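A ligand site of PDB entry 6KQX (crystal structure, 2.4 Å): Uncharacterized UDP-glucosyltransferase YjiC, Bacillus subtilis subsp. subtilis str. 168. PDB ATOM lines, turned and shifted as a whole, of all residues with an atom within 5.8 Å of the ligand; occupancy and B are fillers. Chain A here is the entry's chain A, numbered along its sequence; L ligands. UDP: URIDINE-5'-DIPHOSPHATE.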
ATOM      1  N   TYR A  14     -12.184  -6.168  -3.961  1.00  0.00           N
ATOM      2  CA  TYR A  14     -10.877  -6.724  -4.337  1.00  0.00           C
ATOM      3  C   TYR A  14     -10.518  -6.386  -5.773  1.00  0.00           C
ATOM      4  O   TYR A  14      -9.355  -6.083  -6.069  1.00  0.00           O
ATOM      5  CB  TYR A  14     -10.883  -8.248  -4.146  1.00  0.00           C
ATOM      6  CG  TYR A  14     -10.882  -8.700  -2.708  1.00  0.00           C
ATOM      7  CD1 TYR A  14     -11.970  -8.454  -1.880  1.00  0.00           C
ATOM      8  CD2 TYR A  14      -9.790  -9.379  -2.172  1.00  0.00           C
ATOM      9  CE1 TYR A  14     -11.972  -8.869  -0.563  1.00  0.00           C
ATOM     10  CE2 TYR A  14      -9.786  -9.796  -0.849  1.00  0.00           C
ATOM     11  CZ  TYR A  14     -10.880  -9.539  -0.056  1.00  0.00           C
ATOM     12  OH  TYR A  14     -10.892  -9.943   1.261  1.00  0.00           O
ATOM     13  N   GLY A  15     -11.490  -6.451  -6.689  1.00  0.00           N
ATOM     14  CA  GLY A  15     -11.210  -6.142  -8.081  1.00  0.00           C
ATOM     15  C   GLY A  15     -10.658  -4.745  -8.283  1.00  0.00           C
ATOM     16  O   GLY A  15      -9.973  -4.476  -9.274  1.00  0.00           O
ATOM     17  N   HIS A  16     -10.940  -3.848  -7.346  1.00  0.00           N
ATOM     18  CA  HIS A  16     -10.418  -2.488  -7.389  1.00  0.00           C
ATOM     19  C   HIS A  16      -9.234  -2.268  -6.461  1.00  0.00           C
ATOM     20  O   HIS A  16      -8.366  -1.440  -6.771  1.00  0.00           O
ATOM     21  CB  HIS A  16     -11.527  -1.487  -7.053  1.00  0.00           C
ATOM     22  CG  HIS A  16     -12.743  -1.627  -7.912  1.00  0.00           C
ATOM     23  ND1 HIS A  16     -12.983  -0.807  -8.991  1.00  0.00           N
ATOM     24  CD2 HIS A  16     -13.790  -2.487  -7.852  1.00  0.00           C
ATOM     25  CE1 HIS A  16     -14.122  -1.158  -9.570  1.00  0.00           C
ATOM     26  NE2 HIS A  16     -14.627  -2.180  -8.890  1.00  0.00           N
ATOM     27  N   ASN A  18      -6.934  -4.726  -5.241  1.00  0.00           N
ATOM     28  CA  ASN A  18      -5.753  -5.570  -5.467  1.00  0.00           C
ATOM     29  C   ASN A  18      -4.678  -4.940  -6.342  1.00  0.00           C
ATOM     30  O   ASN A  18      -3.501  -4.957  -5.926  1.00  0.00           O
ATOM     31  CB  ASN A  18      -6.208  -6.924  -6.044  1.00  0.00           C
ATOM     32  CG  ASN A  18      -6.686  -7.879  -4.977  1.00  0.00           C
ATOM     33  OD1 ASN A  18      -6.493  -7.636  -3.781  1.00  0.00           O
ATOM     34  ND2 ASN A  18      -7.292  -8.979  -5.387  1.00  0.00           N
ATOM     35  N   SER A 226     -12.105 -20.553 -11.187  1.00  0.00           N
ATOM     36  CA  SER A 226     -12.524 -19.548 -10.190  1.00  0.00           C
ATOM     37  C   SER A 226     -13.449 -18.522 -10.834  1.00  0.00           C
ATOM     38  O   SER A 226     -13.179 -18.113 -11.970  1.00  0.00           O
ATOM     39  CB  SER A 226     -11.334 -18.890  -9.558  1.00  0.00           C
ATOM     40  OG  SER A 226     -11.685 -17.629  -9.017  1.00  0.00           O
ATOM     41  N   LEU A 227     -14.513 -18.128 -10.128  1.00  0.00           N
ATOM     42  CA  LEU A 227     -15.501 -17.154 -10.675  1.00  0.00           C
ATOM     43  C   LEU A 227     -15.258 -15.789 -10.042  1.00  0.00           C
ATOM     44  O   LEU A 227     -16.163 -14.942 -10.109  1.00  0.00           O
ATOM     45  CB  LEU A 227     -16.914 -17.666 -10.402  1.00  0.00           C
ATOM     46  CG  LEU A 227     -17.403 -18.766 -11.335  1.00  0.00           C
ATOM     47  CD1 LEU A 227     -18.911 -18.862 -11.314  1.00  0.00           C
ATOM     48  CD2 LEU A 227     -16.908 -18.532 -12.750  1.00  0.00           C
ATOM     49  N   GLY A 228     -14.082 -15.577  -9.451  1.00  0.00           N
ATOM     50  CA  GLY A 228     -13.766 -14.262  -8.859  1.00  0.00           C
ATOM     51  C   GLY A 228     -14.152 -14.155  -7.396  1.00  0.00           C
ATOM     52  O   GLY A 228     -14.299 -15.207  -6.741  1.00  0.00           O
ATOM     53  N   THR A 229     -14.350 -12.931  -6.917  1.00  0.00           N
ATOM     54  CA  THR A 229     -14.677 -12.677  -5.491  1.00  0.00           C
ATOM     55  C   THR A 229     -16.053 -12.035  -5.346  1.00  0.00           C
ATOM     56  O   THR A 229     -16.358 -11.569  -4.231  1.00  0.00           O
ATOM     57  CB  THR A 229     -13.625 -11.744  -4.870  1.00  0.00           C
ATOM     58  OG1 THR A 229     -13.685 -11.879  -3.452  1.00  0.00           O
ATOM     59  CG2 THR A 229     -13.830 -10.299  -5.262  1.00  0.00           C
ATOM     60  N   ALA A 230     -16.860 -12.017  -6.412  1.00  0.00           N
ATOM     61  CA  ALA A 230     -18.195 -11.377  -6.316  1.00  0.00           C
ATOM     62  C   ALA A 230     -19.289 -12.307  -6.871  1.00  0.00           C
ATOM     63  O   ALA A 230     -20.217 -12.628  -6.113  1.00  0.00           O
ATOM     64  CB  ALA A 230     -18.181 -10.049  -7.033  1.00  0.00           C
ATOM     65  N   PHE A 231     -19.180 -12.702  -8.142  1.00  0.00           N
ATOM     66  CA  PHE A 231     -20.211 -13.559  -8.771  1.00  0.00           C
ATOM     67  C   PHE A 231     -19.766 -15.025  -8.705  1.00  0.00           C
ATOM     68  O   PHE A 231     -19.757 -15.697  -9.743  1.00  0.00           O
ATOM     69  CB  PHE A 231     -20.464 -13.116 -10.209  1.00  0.00           C
ATOM     70  CG  PHE A 231     -20.644 -11.625 -10.360  1.00  0.00           C
ATOM     71  CD1 PHE A 231     -19.548 -10.783 -10.358  1.00  0.00           C
ATOM     72  CD2 PHE A 231     -21.900 -11.072 -10.497  1.00  0.00           C
ATOM     73  CE1 PHE A 231     -19.706  -9.404 -10.487  1.00  0.00           C
ATOM     74  CE2 PHE A 231     -22.055  -9.701 -10.631  1.00  0.00           C
ATOM     75  CZ  PHE A 231     -20.964  -8.872 -10.630  1.00  0.00           C
ATOM     76  N   SER A 255     -11.497 -22.608  -6.969  1.00  0.00           N
ATOM     77  CA  SER A 255     -11.881 -21.616  -5.940  1.00  0.00           C
ATOM     78  C   SER A 255     -13.407 -21.532  -5.980  1.00  0.00           C
ATOM     79  O   SER A 255     -13.949 -21.146  -7.024  1.00  0.00           O
ATOM     80  CB  SER A 255     -11.245 -20.288  -6.188  1.00  0.00           C
ATOM     81  OG  SER A 255     -11.721 -19.320  -5.266  1.00  0.00           O
ATOM     82  N   GLN A 276     -12.202 -22.298  -0.419  1.00  0.00           N
ATOM     83  CA  GLN A 276     -13.059 -21.093  -0.519  1.00  0.00           C
ATOM     84  C   GLN A 276     -12.256 -19.993  -1.221  1.00  0.00           C
ATOM     85  O   GLN A 276     -12.830 -19.261  -2.038  1.00  0.00           O
ATOM     86  CB  GLN A 276     -13.512 -20.641   0.866  1.00  0.00           C
ATOM     87  CG  GLN A 276     -14.505 -21.590   1.532  1.00  0.00           C
ATOM     88  CD  GLN A 276     -15.552 -20.859   2.342  1.00  0.00           C
ATOM     89  OE1 GLN A 276     -15.263 -19.897   3.038  1.00  0.00           O
ATOM     90  NE2 GLN A 276     -16.786 -21.316   2.233  1.00  0.00           N
ATOM     91  N   SER A 277     -10.969 -19.906  -0.903  1.00  0.00           N
ATOM     92  CA  SER A 277     -10.058 -18.904  -1.517  1.00  0.00           C
ATOM     93  C   SER A 277      -8.766 -19.609  -1.920  1.00  0.00           C
ATOM     94  O   SER A 277      -8.480 -20.674  -1.354  1.00  0.00           O
ATOM     95  CB  SER A 277      -9.795 -17.762  -0.592  1.00  0.00           C
ATOM     96  OG  SER A 277      -8.971 -16.791  -1.215  1.00  0.00           O
ATOM     97  N   VAL A 278      -8.023 -19.027  -2.863  1.00  0.00           N
ATOM     98  CA  VAL A 278      -6.767 -19.672  -3.326  1.00  0.00           C
ATOM     99  C   VAL A 278      -5.783 -18.585  -3.769  1.00  0.00           C
ATOM    100  O   VAL A 278      -6.241 -17.557  -4.282  1.00  0.00           O
ATOM    101  CB  VAL A 278      -7.061 -20.636  -4.487  1.00  0.00           C
ATOM    102  CG1 VAL A 278      -6.375 -20.202  -5.769  1.00  0.00           C
ATOM    103  CG2 VAL A 278      -6.707 -22.074  -4.150  1.00  0.00           C
ATOM    104  N   PRO A 279      -4.457 -18.755  -3.569  1.00  0.00           N
ATOM    105  CA  PRO A 279      -3.484 -17.775  -4.027  1.00  0.00           C
ATOM    106  C   PRO A 279      -3.386 -17.869  -5.552  1.00  0.00           C
ATOM    107  O   PRO A 279      -2.548 -18.589  -6.044  1.00  0.00           O
ATOM    108  CB  PRO A 279      -2.175 -18.240  -3.367  1.00  0.00           C
ATOM    109  CG  PRO A 279      -2.371 -19.726  -3.181  1.00  0.00           C
ATOM    110  CD  PRO A 279      -3.845 -19.900  -2.887  1.00  0.00           C
ATOM    111  N   GLN A 280      -4.261 -17.145  -6.252  1.00  0.00           N
ATOM    112  CA  GLN A 280      -4.361 -17.149  -7.734  1.00  0.00           C
ATOM    113  C   GLN A 280      -2.975 -17.017  -8.368  1.00  0.00           C
ATOM    114  O   GLN A 280      -2.604 -17.892  -9.163  1.00  0.00           O
ATOM    115  CB  GLN A 280      -5.290 -16.021  -8.190  1.00  0.00           C
ATOM    116  CG  GLN A 280      -5.841 -16.228  -9.593  1.00  0.00           C
ATOM    117  CD  GLN A 280      -7.226 -15.649  -9.729  1.00  0.00           C
ATOM    118  OE1 GLN A 280      -8.152 -16.049  -9.036  1.00  0.00           O
ATOM    119  NE2 GLN A 280      -7.366 -14.700 -10.633  1.00  0.00           N
ATOM    120  N   LEU A 281      -2.246 -15.953  -8.017  1.00  0.00           N
ATOM    121  CA  LEU A 281      -0.905 -15.676  -8.587  1.00  0.00           C
ATOM    122  C   LEU A 281      -0.004 -16.917  -8.490  1.00  0.00           C
ATOM    123  O   LEU A 281       0.622 -17.259  -9.509  1.00  0.00           O
ATOM    124  CB  LEU A 281      -0.275 -14.507  -7.831  1.00  0.00           C
ATOM    125  CG  LEU A 281      -0.383 -13.143  -8.506  1.00  0.00           C
ATOM    126  CD1 LEU A 281      -1.793 -12.913  -9.025  1.00  0.00           C
ATOM    127  CD2 LEU A 281       0.008 -12.035  -7.553  1.00  0.00           C
ATOM    128  N   HIS A 293     -13.926 -16.008 -15.104  1.00  0.00           N
ATOM    129  CA  HIS A 293     -15.201 -15.321 -15.273  1.00  0.00           C
ATOM    130  C   HIS A 293     -15.090 -14.000 -16.011  1.00  0.00           C
ATOM    131  O   HIS A 293     -16.112 -13.366 -16.268  1.00  0.00           O
ATOM    132  CB  HIS A 293     -15.854 -15.080 -13.906  1.00  0.00           C
ATOM    133  CG  HIS A 293     -15.197 -13.988 -13.103  1.00  0.00           C
ATOM    134  ND1 HIS A 293     -13.890 -14.068 -12.688  1.00  0.00           N
ATOM    135  CD2 HIS A 293     -15.674 -12.808 -12.640  1.00  0.00           C
ATOM    136  CE1 HIS A 293     -13.584 -12.977 -12.004  1.00  0.00           C
ATOM    137  NE2 HIS A 293     -14.654 -12.196 -11.961  1.00  0.00           N
ATOM    138  N   GLY A 294     -13.882 -13.554 -16.345  1.00  0.00           N
ATOM    139  CA  GLY A 294     -13.723 -12.336 -17.116  1.00  0.00           C
ATOM    140  C   GLY A 294     -13.434 -11.082 -16.331  1.00  0.00           C
ATOM    141  O   GLY A 294     -13.418  -9.993 -16.915  1.00  0.00           O
ATOM    142  N   GLY A 295     -13.234 -11.189 -15.022  1.00  0.00           N
ATOM    143  CA  GLY A 295     -12.730 -10.039 -14.271  1.00  0.00           C
ATOM    144  C   GLY A 295     -11.399  -9.589 -14.838  1.00  0.00           C
ATOM    145  O   GLY A 295     -10.576 -10.396 -15.270  1.00  0.00           O
ATOM    146  N   MET A 296     -11.185  -8.267 -14.847  1.00  0.00           N
ATOM    147  CA  MET A 296      -9.984  -7.720 -15.475  1.00  0.00           C
ATOM    148  C   MET A 296      -8.722  -8.217 -14.791  1.00  0.00           C
ATOM    149  O   MET A 296      -7.740  -8.549 -15.457  1.00  0.00           O
ATOM    150  CB  MET A 296     -10.042  -6.195 -15.469  1.00  0.00           C
ATOM    151  CG  MET A 296      -8.920  -5.539 -16.275  1.00  0.00           C
ATOM    152  SD  MET A 296      -8.802  -6.188 -17.958  1.00  0.00           S
ATOM    153  CE  MET A 296     -10.303  -5.517 -18.677  1.00  0.00           C
ATOM    154  N   ASN A 297      -8.736  -8.287 -13.460  1.00  0.00           N
ATOM    155  CA  ASN A 297      -7.559  -8.745 -12.725  1.00  0.00           C
ATOM    156  C   ASN A 297      -7.195 -10.175 -13.101  1.00  0.00           C
ATOM    157  O   ASN A 297      -6.067 -10.465 -13.509  1.00  0.00           O
ATOM    158  CB  ASN A 297      -7.815  -8.622 -11.215  1.00  0.00           C
ATOM    159  CG  ASN A 297      -7.799  -7.175 -10.745  1.00  0.00           C
ATOM    160  OD1 ASN A 297      -6.750  -6.545 -10.684  1.00  0.00           O
ATOM    161  ND2 ASN A 297      -8.977  -6.658 -10.406  1.00  0.00           N
ATOM    162  N   SER A 298      -8.162 -11.094 -12.983  1.00  0.00           N
ATOM    163  CA  SER A 298      -7.903 -12.502 -13.310  1.00  0.00           C
ATOM    164  C   SER A 298      -7.430 -12.653 -14.749  1.00  0.00           C
ATOM    165  O   SER A 298      -6.524 -13.443 -15.034  1.00  0.00           O
ATOM    166  CB  SER A 298      -9.154 -13.346 -13.059  1.00  0.00           C
ATOM    167  OG  SER A 298      -9.551 -13.304 -11.703  1.00  0.00           O
ATOM    168  N   THR A 299      -8.047 -11.909 -15.668  1.00  0.00           N
ATOM    169  CA  THR A 299      -7.642 -11.966 -17.070  1.00  0.00           C
ATOM    170  C   THR A 299      -6.204 -11.483 -17.243  1.00  0.00           C
ATOM    171  O   THR A 299      -5.392 -12.141 -17.899  1.00  0.00           O
ATOM    172  CB  THR A 299      -8.592 -11.128 -17.919  1.00  0.00           C
ATOM    173  OG1 THR A 299      -9.947 -11.551 -17.691  1.00  0.00           O
ATOM    174  CG2 THR A 299      -8.254 -11.279 -19.394  1.00  0.00           C
ATOM    175  N   GLU A 301      -3.902 -11.248 -14.930  1.00  0.00           N
ATOM    176  CA  GLU A 301      -2.974 -12.123 -14.212  1.00  0.00           C
ATOM    177  C   GLU A 301      -2.713 -13.403 -14.987  1.00  0.00           C
ATOM    178  O   GLU A 301      -1.603 -13.942 -14.945  1.00  0.00           O
ATOM    179  CB  GLU A 301      -3.507 -12.441 -12.820  1.00  0.00           C
ATOM    180  CG  GLU A 301      -3.600 -11.230 -11.903  1.00  0.00           C
ATOM    181  CD  GLU A 301      -4.522 -11.473 -10.713  1.00  0.00           C
ATOM    182  OE1 GLU A 301      -4.944 -12.628 -10.510  1.00  0.00           O
ATOM    183  OE2 GLU A 301      -4.834 -10.501  -9.991  1.00  0.00           O
ATOM    184  N   GLN A 318     -17.601  -8.057 -17.790  1.00  0.00           N
ATOM    185  CA  GLN A 318     -16.944  -9.346 -17.984  1.00  0.00           C
ATOM    186  C   GLN A 318     -17.283  -9.950 -19.337  1.00  0.00           C
ATOM    187  O   GLN A 318     -16.493 -10.718 -19.887  1.00  0.00           O
ATOM    188  CB  GLN A 318     -17.309 -10.289 -16.837  1.00  0.00           C
ATOM    189  CG  GLN A 318     -16.990  -9.702 -15.469  1.00  0.00           C
ATOM    190  CD  GLN A 318     -17.664 -10.429 -14.321  1.00  0.00           C
ATOM    191  OE1 GLN A 318     -18.417 -11.382 -14.538  1.00  0.00           O
ATOM    192  NE2 GLN A 318     -17.426  -9.971 -13.104  1.00  0.00           N
HETATM  193  N1  UDP L   1      -8.479 -13.973  -6.187  1.00  0.00           N
HETATM  194  C2  UDP L   1      -7.595 -14.725  -5.446  1.00  0.00           C
HETATM  195  N3  UDP L   1      -8.061 -15.958  -5.070  1.00  0.00           N
HETATM  196  C4  UDP L   1      -9.304 -16.500  -5.344  1.00  0.00           C
HETATM  197  C5  UDP L   1     -10.162 -15.650  -6.120  1.00  0.00           C
HETATM  198  C6  UDP L   1      -9.736 -14.434  -6.507  1.00  0.00           C
HETATM  199  O2  UDP L   1      -6.473 -14.339  -5.146  1.00  0.00           O
HETATM  200  O4  UDP L   1      -9.583 -17.638  -4.936  1.00  0.00           O
HETATM  201  C1' UDP L   1      -8.030 -12.635  -6.626  1.00  0.00           C
HETATM  202  C2' UDP L   1      -7.498 -12.597  -8.054  1.00  0.00           C
HETATM  203  O2' UDP L   1      -6.109 -12.878  -8.096  1.00  0.00           O
HETATM  204  C3' UDP L   1      -7.778 -11.143  -8.436  1.00  0.00           C
HETATM  205  C4' UDP L   1      -9.119 -10.877  -7.735  1.00  0.00           C
HETATM  206  O4' UDP L   1      -9.148 -11.756  -6.596  1.00  0.00           O
HETATM  207  O3' UDP L   1      -6.774 -10.262  -7.954  1.00  0.00           O
HETATM  208  C5' UDP L   1     -10.341 -11.118  -8.598  1.00  0.00           C
HETATM  209  O5' UDP L   1     -10.768  -9.867  -9.178  1.00  0.00           O
HETATM  210  PA  UDP L   1     -11.298  -9.802 -10.664  1.00  0.00           P
HETATM  211  O1A UDP L   1     -10.620 -10.843 -11.545  1.00  0.00           O
HETATM  212  O2A UDP L   1     -11.200  -8.390 -11.099  1.00  0.00           O
HETATM  213  O3A UDP L   1     -12.828 -10.230 -10.568  1.00  0.00           O
HETATM  214  PB  UDP L   1     -13.823  -9.786  -9.418  1.00  0.00           P
HETATM  215  O1B UDP L   1     -15.196 -10.138  -9.984  1.00  0.00           O
HETATM  216  O2B UDP L   1     -13.476 -10.725  -8.274  1.00  0.00           O
HETATM  217  O3B UDP L   1     -13.673  -8.330  -9.081  1.00  0.00           O
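N of Val 278 is in hydrogen-bond range of O4 of the ligand (2.9 Å).
The backbone carbonyl oxygen (O) of Val 278 lies within hydrogen-bond range of a nitrogen (N3) of the ligand (2.5 Å).
N of Ser 298 sits at hydrogen-bond distance from O1A of the ligand (2.9 Å).
OG of Ser 298 lies within hydrogen-bond range of O1A of the ligand, 2.7 Å away.
OE1 of Glu 301 sits at hydrogen-bond distance from O2' of the ligand (2.7 Å).
N of Thr 229 lies within hydrogen-bond range of O2B of the ligand (2.7 Å).
The side-chain hydroxyl of Ser 255 is in hydrogen-bond range of an oxygen (O4) of the ligand.
An oxygen (O2A) of the ligand sits close to the backbone NH (N) of Asn 297 (3.4 Å).
The side-chain amide nitrogen (ND2) of Asn 297 lies within hydrogen-bond range of an oxygen (O2A) of the ligand, at 2.9 Å.
O1B of the ligand lies within hydrogen-bond range of NE2 of His 293 (2.9 Å).
The side-chain amide nitrogen of Asn 18 is in hydrogen-bond range of an oxygen (O3') of the ligand (2.9 Å).
An oxygen (O2') of the ligand sits close to the side-chain amide nitrogen (NE2) of Gln 280, at 3.4 Å.
OG of Ser 298 sits at hydrogen-bond distance from NE2 of Gln 280, 2.8 Å away.
NE2 of Gln 280 is in hydrogen-bond range of OE1 of Glu 301 (3.2 Å).
The backbone carbonyl oxygen of Gln 276 sits at hydrogen-bond distance from the side-chain hydroxyl of Ser 255, 3.4 Å away.
The side-chain amide nitrogen of Asn 297 sits at hydrogen-bond distance from the backbone carbonyl oxygen of Gly 15.
The backbone carbonyl oxygen (O) of His 293 lies close to the side-chain amide oxygen (OE1) of Gln 318 (3.5 Å).
The backbone carbonyl oxygen of Gly 295 is in hydrogen-bond range of the side-chain hydroxyl of Thr 299, 2.8 Å away.
The backbone NH (N) of Gly 228 is in hydrogen-bond range of the side-chain hydroxyl (OG) of Ser 226, 3.2 Å away.
Merely in contact with the ligand: Gly 15 (3.4 Å), Ser 226 (3.8 Å), Gly 228 (3.6 Å), Ser 277 (3.7 Å), Gly 295 (3.5 Å), Met 296 (3.8 Å) and Gln 318 (3.8 Å).
Hydrophobic or aromatic side chains within 4 Å of the ligand: Val 278 and His 293.
Within 4 Å of the ligand: Gly 15, Asn 18, Ser 226, Gly 228, Thr 229, Ser 255, Ser 277, Val 278, Gln 280, His 293, Gly 295, Met 296, Asn 297, Ser 298, Glu 301 and Gln 318.
The nearest printed residue that does not touch the ligand is Ala 230 (4.1 Å).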
